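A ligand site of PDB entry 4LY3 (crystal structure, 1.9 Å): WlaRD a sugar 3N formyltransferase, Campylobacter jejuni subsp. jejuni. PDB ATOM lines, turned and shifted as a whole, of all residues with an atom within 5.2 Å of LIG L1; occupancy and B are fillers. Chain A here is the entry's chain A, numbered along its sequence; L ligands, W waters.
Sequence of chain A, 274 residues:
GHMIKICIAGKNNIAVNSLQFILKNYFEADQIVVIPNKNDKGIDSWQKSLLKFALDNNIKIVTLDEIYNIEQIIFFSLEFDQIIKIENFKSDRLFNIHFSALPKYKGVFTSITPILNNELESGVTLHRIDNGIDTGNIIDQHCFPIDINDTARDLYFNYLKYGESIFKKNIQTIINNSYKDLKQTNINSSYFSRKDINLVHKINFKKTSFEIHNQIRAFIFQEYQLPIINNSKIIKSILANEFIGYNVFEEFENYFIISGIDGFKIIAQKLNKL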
ATOM      1  N   LYS A  11       1.188   9.430   9.994  1.00  0.00           N
ATOM      2  CA  LYS A  11       0.201  10.513  10.016  1.00  0.00           C
ATOM      3  C   LYS A  11      -1.061  10.156  10.717  1.00  0.00           C
ATOM      4  O   LYS A  11      -1.325   8.989  11.054  1.00  0.00           O
ATOM      5  CB  LYS A  11      -0.100  11.009   8.586  1.00  0.00           C
ATOM      6  CG  LYS A  11      -0.920  10.005   7.783  1.00  0.00           C
ATOM      7  CD  LYS A  11      -1.571  10.569   6.529  1.00  0.00           C
ATOM      8  CE  LYS A  11      -2.432   9.541   5.822  1.00  0.00           C
ATOM      9  NZ  LYS A  11      -2.746  10.033   4.460  1.00  0.00           N
ATOM     10  N   ASN A  12      -1.821  11.212  10.983  1.00  0.00           N
ATOM     11  CA  ASN A  12      -3.175  11.149  11.446  1.00  0.00           C
ATOM     12  C   ASN A  12      -3.288  10.717  12.856  1.00  0.00           C
ATOM     13  O   ASN A  12      -2.290  10.618  13.516  1.00  0.00           O
ATOM     14  CB  ASN A  12      -4.059  10.307  10.504  1.00  0.00           C
ATOM     15  CG  ASN A  12      -4.332  10.988   9.178  1.00  0.00           C
ATOM     16  OD1 ASN A  12      -3.930  12.133   8.915  1.00  0.00           O
ATOM     17  ND2 ASN A  12      -4.967  10.242   8.291  1.00  0.00           N
ATOM     18  N   ASN A  37       4.499  12.444   7.006  1.00  0.00           N
ATOM     19  CA  ASN A  37       4.326  12.222   5.586  1.00  0.00           C
ATOM     20  C   ASN A  37       4.537  13.528   4.798  1.00  0.00           C
ATOM     21  O   ASN A  37       4.426  14.640   5.344  1.00  0.00           O
ATOM     22  CB  ASN A  37       2.925  11.680   5.335  1.00  0.00           C
ATOM     23  CG  ASN A  37       2.776  10.227   5.715  1.00  0.00           C
ATOM     24  OD1 ASN A  37       3.670   9.586   6.277  1.00  0.00           O
ATOM     25  ND2 ASN A  37       1.617   9.680   5.377  1.00  0.00           N
ATOM     26  N   SER A  77       5.998   2.518  11.648  1.00  0.00           N
ATOM     27  CA  SER A  77       5.167   3.142  10.620  1.00  0.00           C
ATOM     28  C   SER A  77       3.672   3.085  10.996  1.00  0.00           C
ATOM     29  O   SER A  77       3.116   2.044  11.341  1.00  0.00           O
ATOM     30  CB  SER A  77       5.366   2.456   9.254  1.00  0.00           C
ATOM     31  OG  SER A  77       4.287   2.779   8.372  1.00  0.00           O
ATOM     32  N   GLU A  79       0.588   4.663   9.141  1.00  0.00           N
ATOM     33  CA  GLU A  79       0.180   5.285   7.908  1.00  0.00           C
ATOM     34  C   GLU A  79       1.263   6.089   7.225  1.00  0.00           C
ATOM     35  O   GLU A  79       1.031   7.111   6.557  1.00  0.00           O
ATOM     36  CB  GLU A  79      -1.133   6.087   8.162  1.00  0.00           C
ATOM     37  CG  GLU A  79      -2.283   5.214   8.586  1.00  0.00           C
ATOM     38  CD  GLU A  79      -2.510   4.020   7.667  1.00  0.00           C
ATOM     39  OE1 GLU A  79      -2.985   4.237   6.511  1.00  0.00           O
ATOM     40  OE2 GLU A  79      -2.248   2.891   8.176  1.00  0.00           O
ATOM     41  N   PHE A  80       2.479   5.531   7.249  1.00  0.00           N
ATOM     42  CA  PHE A  80       3.607   6.213   6.633  1.00  0.00           C
ATOM     43  C   PHE A  80       3.532   6.035   5.128  1.00  0.00           C
ATOM     44  O   PHE A  80       3.087   4.992   4.646  1.00  0.00           O
ATOM     45  CB  PHE A  80       4.889   5.605   7.203  1.00  0.00           C
ATOM     46  CG  PHE A  80       6.167   6.251   6.781  1.00  0.00           C
ATOM     47  CD1 PHE A  80       7.267   5.478   6.416  1.00  0.00           C
ATOM     48  CD2 PHE A  80       6.328   7.630   6.818  1.00  0.00           C
ATOM     49  CE1 PHE A  80       8.486   6.061   6.078  1.00  0.00           C
ATOM     50  CE2 PHE A  80       7.525   8.230   6.465  1.00  0.00           C
ATOM     51  CZ  PHE A  80       8.614   7.440   6.091  1.00  0.00           C
ATOM     52  N   ASP A  81       4.029   7.017   4.421  1.00  0.00           N
ATOM     53  CA  ASP A  81       3.842   7.169   2.977  1.00  0.00           C
ATOM     54  C   ASP A  81       5.002   6.675   2.132  1.00  0.00           C
ATOM     55  O   ASP A  81       4.942   6.829   0.949  1.00  0.00           O
ATOM     56  CB  ASP A  81       3.459   8.604   2.572  1.00  0.00           C
ATOM     57  CG  ASP A  81       4.571   9.663   2.782  1.00  0.00           C
ATOM     58  OD1 ASP A  81       4.441  10.819   2.307  1.00  0.00           O
ATOM     59  OD2 ASP A  81       5.627   9.382   3.331  1.00  0.00           O
ATOM     60  N   ASN A  96       4.989  -1.982  11.411  1.00  0.00           N
ATOM     61  CA  ASN A  96       3.933  -1.280  10.690  1.00  0.00           C
ATOM     62  C   ASN A  96       2.609  -1.757  11.219  1.00  0.00           C
ATOM     63  O   ASN A  96       2.480  -2.904  11.643  1.00  0.00           O
ATOM     64  CB  ASN A  96       3.979  -1.534   9.170  1.00  0.00           C
ATOM     65  CG  ASN A  96       2.805  -0.900   8.428  1.00  0.00           C
ATOM     66  OD1 ASN A  96       1.982  -1.559   7.738  1.00  0.00           O
ATOM     67  ND2 ASN A  96       2.763   0.406   8.497  1.00  0.00           N
ATOM     68  N   HIS A  98      -0.949  -2.105   9.534  1.00  0.00           N
ATOM     69  CA  HIS A  98      -1.654  -2.088   8.239  1.00  0.00           C
ATOM     70  C   HIS A  98      -3.142  -2.177   8.515  1.00  0.00           C
ATOM     71  O   HIS A  98      -3.590  -3.034   9.268  1.00  0.00           O
ATOM     72  CB  HIS A  98      -1.199  -3.187   7.320  1.00  0.00           C
ATOM     73  CG  HIS A  98      -1.878  -3.185   5.976  1.00  0.00           C
ATOM     74  ND1 HIS A  98      -1.622  -2.243   5.012  1.00  0.00           N
ATOM     75  CD2 HIS A  98      -2.843  -3.985   5.474  1.00  0.00           C
ATOM     76  CE1 HIS A  98      -2.387  -2.473   3.962  1.00  0.00           C
ATOM     77  NE2 HIS A  98      -3.159  -3.502   4.229  1.00  0.00           N
ATOM     78  N   GLY A 107      -1.624  -3.407   0.236  1.00  0.00           N
ATOM     79  CA  GLY A 107      -1.609  -2.243  -0.611  1.00  0.00           C
ATOM     80  C   GLY A 107      -2.466  -1.131  -0.084  1.00  0.00           C
ATOM     81  O   GLY A 107      -2.509  -0.909   1.105  1.00  0.00           O
ATOM     82  N   VAL A 108      -3.163  -0.416  -0.968  1.00  0.00           N
ATOM     83  CA  VAL A 108      -3.693   0.899  -0.659  1.00  0.00           C
ATOM     84  C   VAL A 108      -5.246   0.915  -0.703  1.00  0.00           C
ATOM     85  O   VAL A 108      -5.951  -0.069  -1.063  1.00  0.00           O
ATOM     86  CB  VAL A 108      -3.062   1.978  -1.594  1.00  0.00           C
ATOM     87  CG1 VAL A 108      -1.516   1.967  -1.463  1.00  0.00           C
ATOM     88  CG2 VAL A 108      -3.453   1.725  -3.042  1.00  0.00           C
ATOM     89  N   PHE A 109      -5.762   2.066  -0.318  1.00  0.00           N
ATOM     90  CA  PHE A 109      -7.208   2.308  -0.411  1.00  0.00           C
ATOM     91  C   PHE A 109      -7.998   1.248   0.352  1.00  0.00           C
ATOM     92  O   PHE A 109      -9.087   0.847  -0.059  1.00  0.00           O
ATOM     93  CB  PHE A 109      -7.593   2.367  -1.894  1.00  0.00           C
ATOM     94  CG  PHE A 109      -7.091   3.575  -2.629  1.00  0.00           C
ATOM     95  CD1 PHE A 109      -6.827   3.504  -3.972  1.00  0.00           C
ATOM     96  CD2 PHE A 109      -6.960   4.796  -2.011  1.00  0.00           C
ATOM     97  CE1 PHE A 109      -6.417   4.605  -4.690  1.00  0.00           C
ATOM     98  CE2 PHE A 109      -6.549   5.905  -2.723  1.00  0.00           C
ATOM     99  CZ  PHE A 109      -6.250   5.804  -4.055  1.00  0.00           C
ATOM    100  N   THR A 110      -7.531   0.863   1.532  1.00  0.00           N
ATOM    101  CA  THR A 110      -8.085  -0.284   2.254  1.00  0.00           C
ATOM    102  C   THR A 110      -9.415   0.024   2.979  1.00  0.00           C
ATOM    103  O   THR A 110     -10.027  -0.881   3.591  1.00  0.00           O
ATOM    104  CB  THR A 110      -7.139  -0.890   3.300  1.00  0.00           C
ATOM    105  OG1 THR A 110      -6.848   0.077   4.326  1.00  0.00           O
ATOM    106  CG2 THR A 110      -5.808  -1.293   2.683  1.00  0.00           C
ATOM    107  N   SER A 111      -9.814   1.277   2.950  1.00  0.00           N
ATOM    108  CA  SER A 111     -11.149   1.608   3.374  1.00  0.00           C
ATOM    109  C   SER A 111     -12.149   1.438   2.228  1.00  0.00           C
ATOM    110  O   SER A 111     -13.357   1.394   2.503  1.00  0.00           O
ATOM    111  CB  SER A 111     -11.204   3.021   3.918  1.00  0.00           C
ATOM    112  OG  SER A 111     -10.414   3.074   5.087  1.00  0.00           O
ATOM    113  N   ILE A 112     -11.651   1.328   0.988  1.00  0.00           N
ATOM    114  CA  ILE A 112     -12.494   1.062  -0.203  1.00  0.00           C
ATOM    115  C   ILE A 112     -12.558  -0.430  -0.528  1.00  0.00           C
ATOM    116  O   ILE A 112     -13.626  -1.055  -0.598  1.00  0.00           O
ATOM    117  CB  ILE A 112     -12.013   1.895  -1.393  1.00  0.00           C
ATOM    118  CG1 ILE A 112     -11.951   3.357  -0.988  1.00  0.00           C
ATOM    119  CG2 ILE A 112     -12.866   1.656  -2.644  1.00  0.00           C
ATOM    120  CD1 ILE A 112     -11.452   4.279  -2.070  1.00  0.00           C
ATOM    121  N   ASP A 134       3.357  -4.798   2.829  1.00  0.00           N
ATOM    122  CA  ASP A 134       2.425  -5.407   3.794  1.00  0.00           C
ATOM    123  C   ASP A 134       2.529  -6.904   3.868  1.00  0.00           C
ATOM    124  O   ASP A 134       1.550  -7.609   4.206  1.00  0.00           O
ATOM    125  CB  ASP A 134       0.966  -5.006   3.525  1.00  0.00           C
ATOM    126  CG  ASP A 134       0.772  -3.506   3.451  1.00  0.00           C
ATOM    127  OD1 ASP A 134       1.420  -2.778   4.234  1.00  0.00           O
ATOM    128  OD2 ASP A 134      -0.007  -3.055   2.577  1.00  0.00           O
ATOM    129  N   TYR A 156     -12.652   3.720   7.818  1.00  0.00           N
ATOM    130  CA  TYR A 156     -11.406   4.358   8.097  1.00  0.00           C
ATOM    131  C   TYR A 156     -11.322   4.806   9.553  1.00  0.00           C
ATOM    132  O   TYR A 156     -10.304   4.639  10.225  1.00  0.00           O
ATOM    133  CB  TYR A 156     -11.150   5.495   7.125  1.00  0.00           C
ATOM    134  CG  TYR A 156      -9.759   6.050   7.286  1.00  0.00           C
ATOM    135  CD1 TYR A 156      -8.658   5.329   6.847  1.00  0.00           C
ATOM    136  CD2 TYR A 156      -9.528   7.270   7.901  1.00  0.00           C
ATOM    137  CE1 TYR A 156      -7.372   5.797   7.006  1.00  0.00           C
ATOM    138  CE2 TYR A 156      -8.226   7.763   8.058  1.00  0.00           C
ATOM    139  CZ  TYR A 156      -7.128   7.012   7.623  1.00  0.00           C
ATOM    140  OH  TYR A 156      -5.820   7.514   7.770  1.00  0.00           O
ATOM    141  N   ARG A 194      -2.783   1.622  -6.593  1.00  0.00           N
ATOM    142  CA  ARG A 194      -3.536   2.840  -6.907  1.00  0.00           C
ATOM    143  C   ARG A 194      -4.225   2.694  -8.220  1.00  0.00           C
ATOM    144  O   ARG A 194      -5.383   2.991  -8.340  1.00  0.00           O
ATOM    145  CB  ARG A 194      -2.619   4.055  -6.957  1.00  0.00           C
ATOM    146  CG  ARG A 194      -2.243   4.444  -5.552  1.00  0.00           C
ATOM    147  CD  ARG A 194      -1.670   5.844  -5.408  1.00  0.00           C
ATOM    148  NE  ARG A 194      -1.281   5.982  -3.996  1.00  0.00           N
ATOM    149  CZ  ARG A 194      -0.058   5.760  -3.516  1.00  0.00           C
ATOM    150  NH1 ARG A 194       0.970   5.476  -4.329  1.00  0.00           N
ATOM    151  NH2 ARG A 194       0.146   5.881  -2.201  1.00  0.00           N
ATOM    152  N   LEU A 199     -11.093   6.201  -8.549  1.00  0.00           N
ATOM    153  CA  LEU A 199     -11.734   6.947  -7.469  1.00  0.00           C
ATOM    154  C   LEU A 199     -12.999   7.652  -7.954  1.00  0.00           C
ATOM    155  O   LEU A 199     -13.791   8.094  -7.109  1.00  0.00           O
ATOM    156  CB  LEU A 199     -10.777   7.953  -6.833  1.00  0.00           C
ATOM    157  CG  LEU A 199      -9.571   7.370  -6.094  1.00  0.00           C
ATOM    158  CD1 LEU A 199      -8.417   8.344  -5.933  1.00  0.00           C
ATOM    159  CD2 LEU A 199      -9.974   6.776  -4.762  1.00  0.00           C
ATOM    160  N   PHE A 219     -17.159   4.295  -1.835  1.00  0.00           N
ATOM    161  CA  PHE A 219     -16.585   5.552  -2.335  1.00  0.00           C
ATOM    162  C   PHE A 219     -17.038   6.791  -1.591  1.00  0.00           C
ATOM    163  O   PHE A 219     -16.693   7.917  -1.944  1.00  0.00           O
ATOM    164  CB  PHE A 219     -16.875   5.653  -3.808  1.00  0.00           C
ATOM    165  CG  PHE A 219     -16.010   4.720  -4.630  1.00  0.00           C
ATOM    166  CD1 PHE A 219     -14.674   5.073  -4.916  1.00  0.00           C
ATOM    167  CD2 PHE A 219     -16.482   3.481  -4.993  1.00  0.00           C
ATOM    168  CE1 PHE A 219     -13.846   4.210  -5.612  1.00  0.00           C
ATOM    169  CE2 PHE A 219     -15.685   2.604  -5.714  1.00  0.00           C
ATOM    170  CZ  PHE A 219     -14.367   2.976  -6.031  1.00  0.00           C
ATOM    171  N   PHE A 221     -16.512   9.098   1.041  1.00  0.00           N
ATOM    172  CA  PHE A 221     -15.461   9.600   1.938  1.00  0.00           C
ATOM    173  C   PHE A 221     -15.284  11.073   1.607  1.00  0.00           C
ATOM    174  O   PHE A 221     -14.474  11.445   0.751  1.00  0.00           O
ATOM    175  CB  PHE A 221     -14.173   8.821   1.740  1.00  0.00           C
ATOM    176  CG  PHE A 221     -13.232   8.870   2.945  1.00  0.00           C
ATOM    177  CD1 PHE A 221     -12.584   7.709   3.352  1.00  0.00           C
ATOM    178  CD2 PHE A 221     -13.070  10.016   3.718  1.00  0.00           C
ATOM    179  CE1 PHE A 221     -11.715   7.707   4.446  1.00  0.00           C
ATOM    180  CE2 PHE A 221     -12.184  10.018   4.803  1.00  0.00           C
ATOM    181  CZ  PHE A 221     -11.515   8.854   5.179  1.00  0.00           C
ATOM    182  N   TYR A 224     -12.585  13.434   0.530  1.00  0.00           N
ATOM    183  CA  TYR A 224     -11.950  13.166  -0.755  1.00  0.00           C
ATOM    184  C   TYR A 224     -12.929  13.217  -1.897  1.00  0.00           C
ATOM    185  O   TYR A 224     -12.711  13.934  -2.858  1.00  0.00           O
ATOM    186  CB  TYR A 224     -11.340  11.749  -0.735  1.00  0.00           C
ATOM    187  CG  TYR A 224     -10.188  11.621   0.231  1.00  0.00           C
ATOM    188  CD1 TYR A 224      -8.977  12.187  -0.056  1.00  0.00           C
ATOM    189  CD2 TYR A 224     -10.346  10.965   1.431  1.00  0.00           C
ATOM    190  CE1 TYR A 224      -7.901  12.109   0.839  1.00  0.00           C
ATOM    191  CE2 TYR A 224      -9.311  10.914   2.349  1.00  0.00           C
ATOM    192  CZ  TYR A 224      -8.065  11.480   2.039  1.00  0.00           C
ATOM    193  OH  TYR A 224      -7.013  11.383   2.945  1.00  0.00           O
ATOM    194  N   GLN A 225     -13.953  12.369  -1.830  1.00  0.00           N
ATOM    195  CA  GLN A 225     -14.962  12.340  -2.876  1.00  0.00           C
ATOM    196  C   GLN A 225     -16.237  11.686  -2.400  1.00  0.00           C
ATOM    197  O   GLN A 225     -16.334  11.052  -1.328  1.00  0.00           O
ATOM    198  CB  GLN A 225     -14.433  11.703  -4.179  1.00  0.00           C
ATOM    199  CG  GLN A 225     -14.382  10.167  -4.218  1.00  0.00           C
ATOM    200  CD  GLN A 225     -13.355   9.557  -3.292  1.00  0.00           C
ATOM    201  OE1 GLN A 225     -12.141   9.840  -3.411  1.00  0.00           O
ATOM    202  NE2 GLN A 225     -13.821   8.759  -2.326  1.00  0.00           N
HETATM  203  O1  LIG L   1      -8.594  10.113  -2.965  1.00  0.00           O
HETATM  204  C1  LIG L   1      -8.901   9.364  -1.994  1.00  0.00           C
HETATM  205  N1  LIG L   1     -10.166   8.925  -1.841  1.00  0.00           N
HETATM  206  C2  LIG L   1     -10.470   8.175  -0.763  1.00  0.00           C
HETATM  207  O2  LIG L   1     -11.681   7.756  -0.704  1.00  0.00           O
HETATM  208  C3  LIG L   1      -7.952   9.005  -1.046  1.00  0.00           C
HETATM  209  C4  LIG L   1      -6.551   9.559  -1.237  1.00  0.00           C
HETATM  210  C5  LIG L   1      -8.287   8.291  -0.020  1.00  0.00           C
HETATM  211  N2  LIG L   1      -9.524   7.867   0.128  1.00  0.00           N
HETATM  212  C6  LIG L   1      -9.860   7.021   1.288  1.00  0.00           C
HETATM  213  O3  LIG L   1      -9.076   7.413   2.409  1.00  0.00           O
HETATM  214  C7  LIG L   1      -9.543   5.560   1.005  1.00  0.00           C
HETATM  215  C8  LIG L   1      -8.351   5.224   1.909  1.00  0.00           C
HETATM  216  O4  LIG L   1      -8.386   3.902   2.407  1.00  0.00           O
HETATM  217  C9  LIG L   1      -8.438   6.291   2.988  1.00  0.00           C
HETATM  218  C10 LIG L   1      -7.081   6.726   3.536  1.00  0.00           C
HETATM  219  O5  LIG L   1      -6.339   7.310   2.484  1.00  0.00           O
HETATM  220  P1  LIG L   1      -4.744   7.346   2.522  1.00  0.00           P
HETATM  221  O6  LIG L   1      -4.432   7.908   3.894  1.00  0.00           O
HETATM  222  O7  LIG L   1      -4.298   7.941   1.211  1.00  0.00           O
HETATM  223  O8  LIG L   1      -4.295   5.847   2.818  1.00  0.00           O
HETATM  224  P2  LIG L   1      -4.657   4.433   2.114  1.00  0.00           P
HETATM  225  O9  LIG L   1      -5.879   3.759   2.800  1.00  0.00           O
HETATM  226  O10 LIG L   1      -4.401   4.521   0.654  1.00  0.00           O
HETATM  227  O11 LIG L   1      -3.368   3.746   2.787  1.00  0.00           O
HETATM  228  O12 LIG L   1       0.599   4.231   5.104  1.00  0.00           O
HETATM  229  C11 LIG L   1       0.068   4.054   3.779  1.00  0.00           C
HETATM  230  C12 LIG L   1      -0.832   5.192   3.297  1.00  0.00           C
HETATM  231  O13 LIG L   1      -1.360   4.820   2.009  1.00  0.00           O
HETATM  232  C13 LIG L   1      -0.207   6.570   3.197  1.00  0.00           C
HETATM  233  C14 LIG L   1      -0.793   2.835   3.929  1.00  0.00           C
HETATM  234  N3  LIG L   1      -0.042   1.744   4.526  1.00  0.00           N
HETATM  235  C15 LIG L   1      -1.361   2.434   2.562  1.00  0.00           C
HETATM  236  O14 LIG L   1      -2.223   1.301   2.752  1.00  0.00           O
HETATM  237  C16 LIG L   1      -2.152   3.632   2.004  1.00  0.00           C
HETATM  238  N1  LG2 L   2       6.927  -2.717   3.739  1.00  0.00           N
HETATM  239  C1  LG2 L   2       7.839  -1.817   3.345  1.00  0.00           C
HETATM  240  N2  LG2 L   2       7.727  -0.492   3.620  1.00  0.00           N
HETATM  241  C2  LG2 L   2       6.616  -0.071   4.264  1.00  0.00           C
HETATM  242  C3  LG2 L   2       5.611  -0.977   4.621  1.00  0.00           C
HETATM  243  C4  LG2 L   2       5.778  -2.326   4.333  1.00  0.00           C
HETATM  244  N3  LG2 L   2       6.522   1.236   4.495  1.00  0.00           N
HETATM  245  C5  LG2 L   2       5.284   1.716   5.158  1.00  0.00           C
HETATM  246  C6  LG2 L   2       4.042   0.809   4.984  1.00  0.00           C
HETATM  247  N4  LG2 L   2       4.452  -0.552   5.209  1.00  0.00           N
HETATM  248  C7  LG2 L   2       3.277   0.764   3.649  1.00  0.00           C
HETATM  249  N5  LG2 L   2       3.169   2.022   2.948  1.00  0.00           N
HETATM  250  C8  LG2 L   2       2.905   2.170   1.630  1.00  0.00           C
HETATM  251  C9  LG2 L   2       3.370   3.354   1.051  1.00  0.00           C
HETATM  252  C10 LG2 L   2       3.220   3.621  -0.302  1.00  0.00           C
HETATM  253  C11 LG2 L   2       2.607   2.676  -1.137  1.00  0.00           C
HETATM  254  C12 LG2 L   2       2.150   1.487  -0.569  1.00  0.00           C
HETATM  255  C13 LG2 L   2       2.304   1.213   0.791  1.00  0.00           C
HETATM  256  C14 LG2 L   2       2.543   3.006  -2.594  1.00  0.00           C
HETATM  257  N6  LG2 L   2       2.109   2.144  -3.512  1.00  0.00           N
HETATM  258  C15 LG2 L   2       2.067   2.369  -4.947  1.00  0.00           C
HETATM  259  C16 LG2 L   2       0.717   2.314  -5.621  1.00  0.00           C
HETATM  260  O1  LG2 L   2      -0.231   1.657  -5.115  1.00  0.00           O
HETATM  261  O2  LG2 L   2       0.624   2.944  -6.695  1.00  0.00           O
HETATM  262  C17 LG2 L   2       2.830   1.187  -5.544  1.00  0.00           C
HETATM  263  C18 LG2 L   2       4.327   1.352  -5.312  1.00  0.00           C
HETATM  264  C19 LG2 L   2       5.145   0.211  -5.890  1.00  0.00           C
HETATM  265  O3  LG2 L   2       6.357   0.219  -5.547  1.00  0.00           O
HETATM  266  O4  LG2 L   2       4.623  -0.650  -6.654  1.00  0.00           O
HETATM  267  O5  LG2 L   2       3.013   4.101  -2.906  1.00  0.00           O
HETATM  268  O6  LG2 L   2       4.914  -3.325   4.659  1.00  0.00           O
HETATM  269  N7  LG2 L   2       8.966  -2.292   2.760  1.00  0.00           N
HETATM  270  O   HOH W   1       0.515  -0.541   5.402  1.00  0.00           O
HETATM  271  O   HOH W   2       0.536   1.894   7.592  1.00  0.00           O
HETATM  272  O   HOH W   3      -4.088   6.623   6.210  1.00  0.00           O
HETATM  273  O   HOH W   4      -6.337  10.749  -4.301  1.00  0.00           O
HETATM  274  O   HOH W   5       0.070  -0.372   2.740  1.00  0.00           O
HETATM  275  O   HOH W   6      -2.508   0.731   6.484  1.00  0.00           O
HETATM  276  O   HOH W   7      -5.699  10.333   5.273  1.00  0.00           O
HETATM  277  O   HOH W   8      -3.409   6.125  -0.887  1.00  0.00           O
HETATM  278  O   HOH W   9      -7.540   2.619   4.923  1.00  0.00           O
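The backbone NH of Phe 80 sits at hydrogen-bond distance from an oxygen (O12) of LIG L1 (3.1 Å).
O of Phe 80 lies within hydrogen-bond range of O12 of LIG L1 (2.6 Å).
OE1 of Gln 225 sits at hydrogen-bond distance from N1 of LIG L1, 2.7 Å away.
An oxygen (O14) of LIG L1 sits at hydrogen-bond distance from the backbone carbonyl oxygen (O) of Gly 107, at 2.8 Å.
The side-chain amino group (NZ) of Lys 11 lies within salt-bridge range of an oxygen (O6) of LIG L1 (2.8 Å).
O of Glu 79 sits close to O12 of LIG L1.
N of Phe 109 lies within hydrogen-bond range of O10 of LIG L1 (3.0 Å).
The backbone NH (N) of Ser 111 sits at hydrogen-bond distance from an oxygen (O4) of LIG L1 (3.0 Å).
The side-chain hydroxyl of Ser 111 sits close to an oxygen (O4) of LIG L1, 3.5 Å away.
N of Thr 110 is in hydrogen-bond range of O4 of LIG L1, at 3.3 Å.
The backbone carbonyl oxygen of Phe 80 is in hydrogen-bond range of a nitrogen (N5) of LG2 L2 (3.4 Å).
The backbone NH (N) of Arg 194 is in hydrogen-bond range of an oxygen (O1) of LG2 L2, at 2.9 Å.
The guanidinium group (NH1) of Arg 194 is in salt-bridge range of an oxygen (O2) of LG2 L2 (3.5 Å).
The backbone NH (N) of Asp 134 lies within hydrogen-bond range of an oxygen (O6) of LG2 L2, at 2.8 Å.
N of Phe 80 lies close to OG of Ser 77, 3.5 Å away.
NE2 of Gln 225 sits at hydrogen-bond distance from O of Phe 219 (3.0 Å).
N of Gly 107 lies within hydrogen-bond range of OD2 of Asp 134 (2.9 Å).
The backbone carbonyl oxygen of Glu 79 sits at hydrogen-bond distance from the side-chain amide nitrogen of Asn 37 (2.9 Å).
OH of Tyr 156 lies within hydrogen-bond range of ND2 of Asn 12.
OD2 of Asp 134 sits close to ND1 of His 98.
The side-chain amide oxygen (OD1) of Asn 96 sits at hydrogen-bond distance from the backbone NH (N) of His 98.
Merely in contact with LIG L1: His 98, Val 108, Ile 112, Tyr 156, Leu 199, Phe 221 and Tyr 224.
Hydrophobic or aromatic side chains that line LIG L1: His 98, Val 108, Phe 109, Ile 112, Tyr 156, Leu 199, Phe 221 and Tyr 224.
15 residues have an atom within 4 Å of LIG L1: Lys 11, Glu 79, Phe 80, His 98, Gly 107, Val 108, Phe 109, Thr 110, Ser 111, Ile 112, Tyr 156, Leu 199, Phe 221, Tyr 224 and Gln 225.
The nearest printed residue that does not touch LIG L1 is Asp 81 (4.1 Å).
Water W3 lies within hydrogen-bond range of OH of Tyr 156 (2.5 Å), OE1 of Glu 79 (2.6 Å) and O6 of LIG L1 (2.7 Å).
Water W5 lies within hydrogen-bond range of OD2 of Asp 134 (2.7 Å), N3 of LIG L1 (2.8 Å), O of Gly 107 (3.1 Å) and ND1 of His 98 (3.4 Å).
Water W9 lies within hydrogen-bond range of the side-chain hydroxyl of Thr 110 (2.7 Å), the side-chain hydroxyl of Ser 111 (2.9 Å) and an oxygen (O9) of LIG L1 (2.9 Å).
Water W7 lies within hydrogen-bond range of the side-chain hydroxyl (OH) of Tyr 224 (2.9 Å), an oxygen (O6) of LIG L1 (3.1 Å), the side-chain amino group (NZ) of Lys 11 (3.1 Å) and the side-chain amide nitrogen (ND2) of Asn 12 (3.1 Å).
Water W2 lies within hydrogen-bond range of ND2 of Asn 96, OE2 of Glu 79 and N3 of LIG L1.
Water W6 lies within hydrogen-bond range of OE2 of Glu 79, N3 of LIG L1 and ND1 of His 98.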
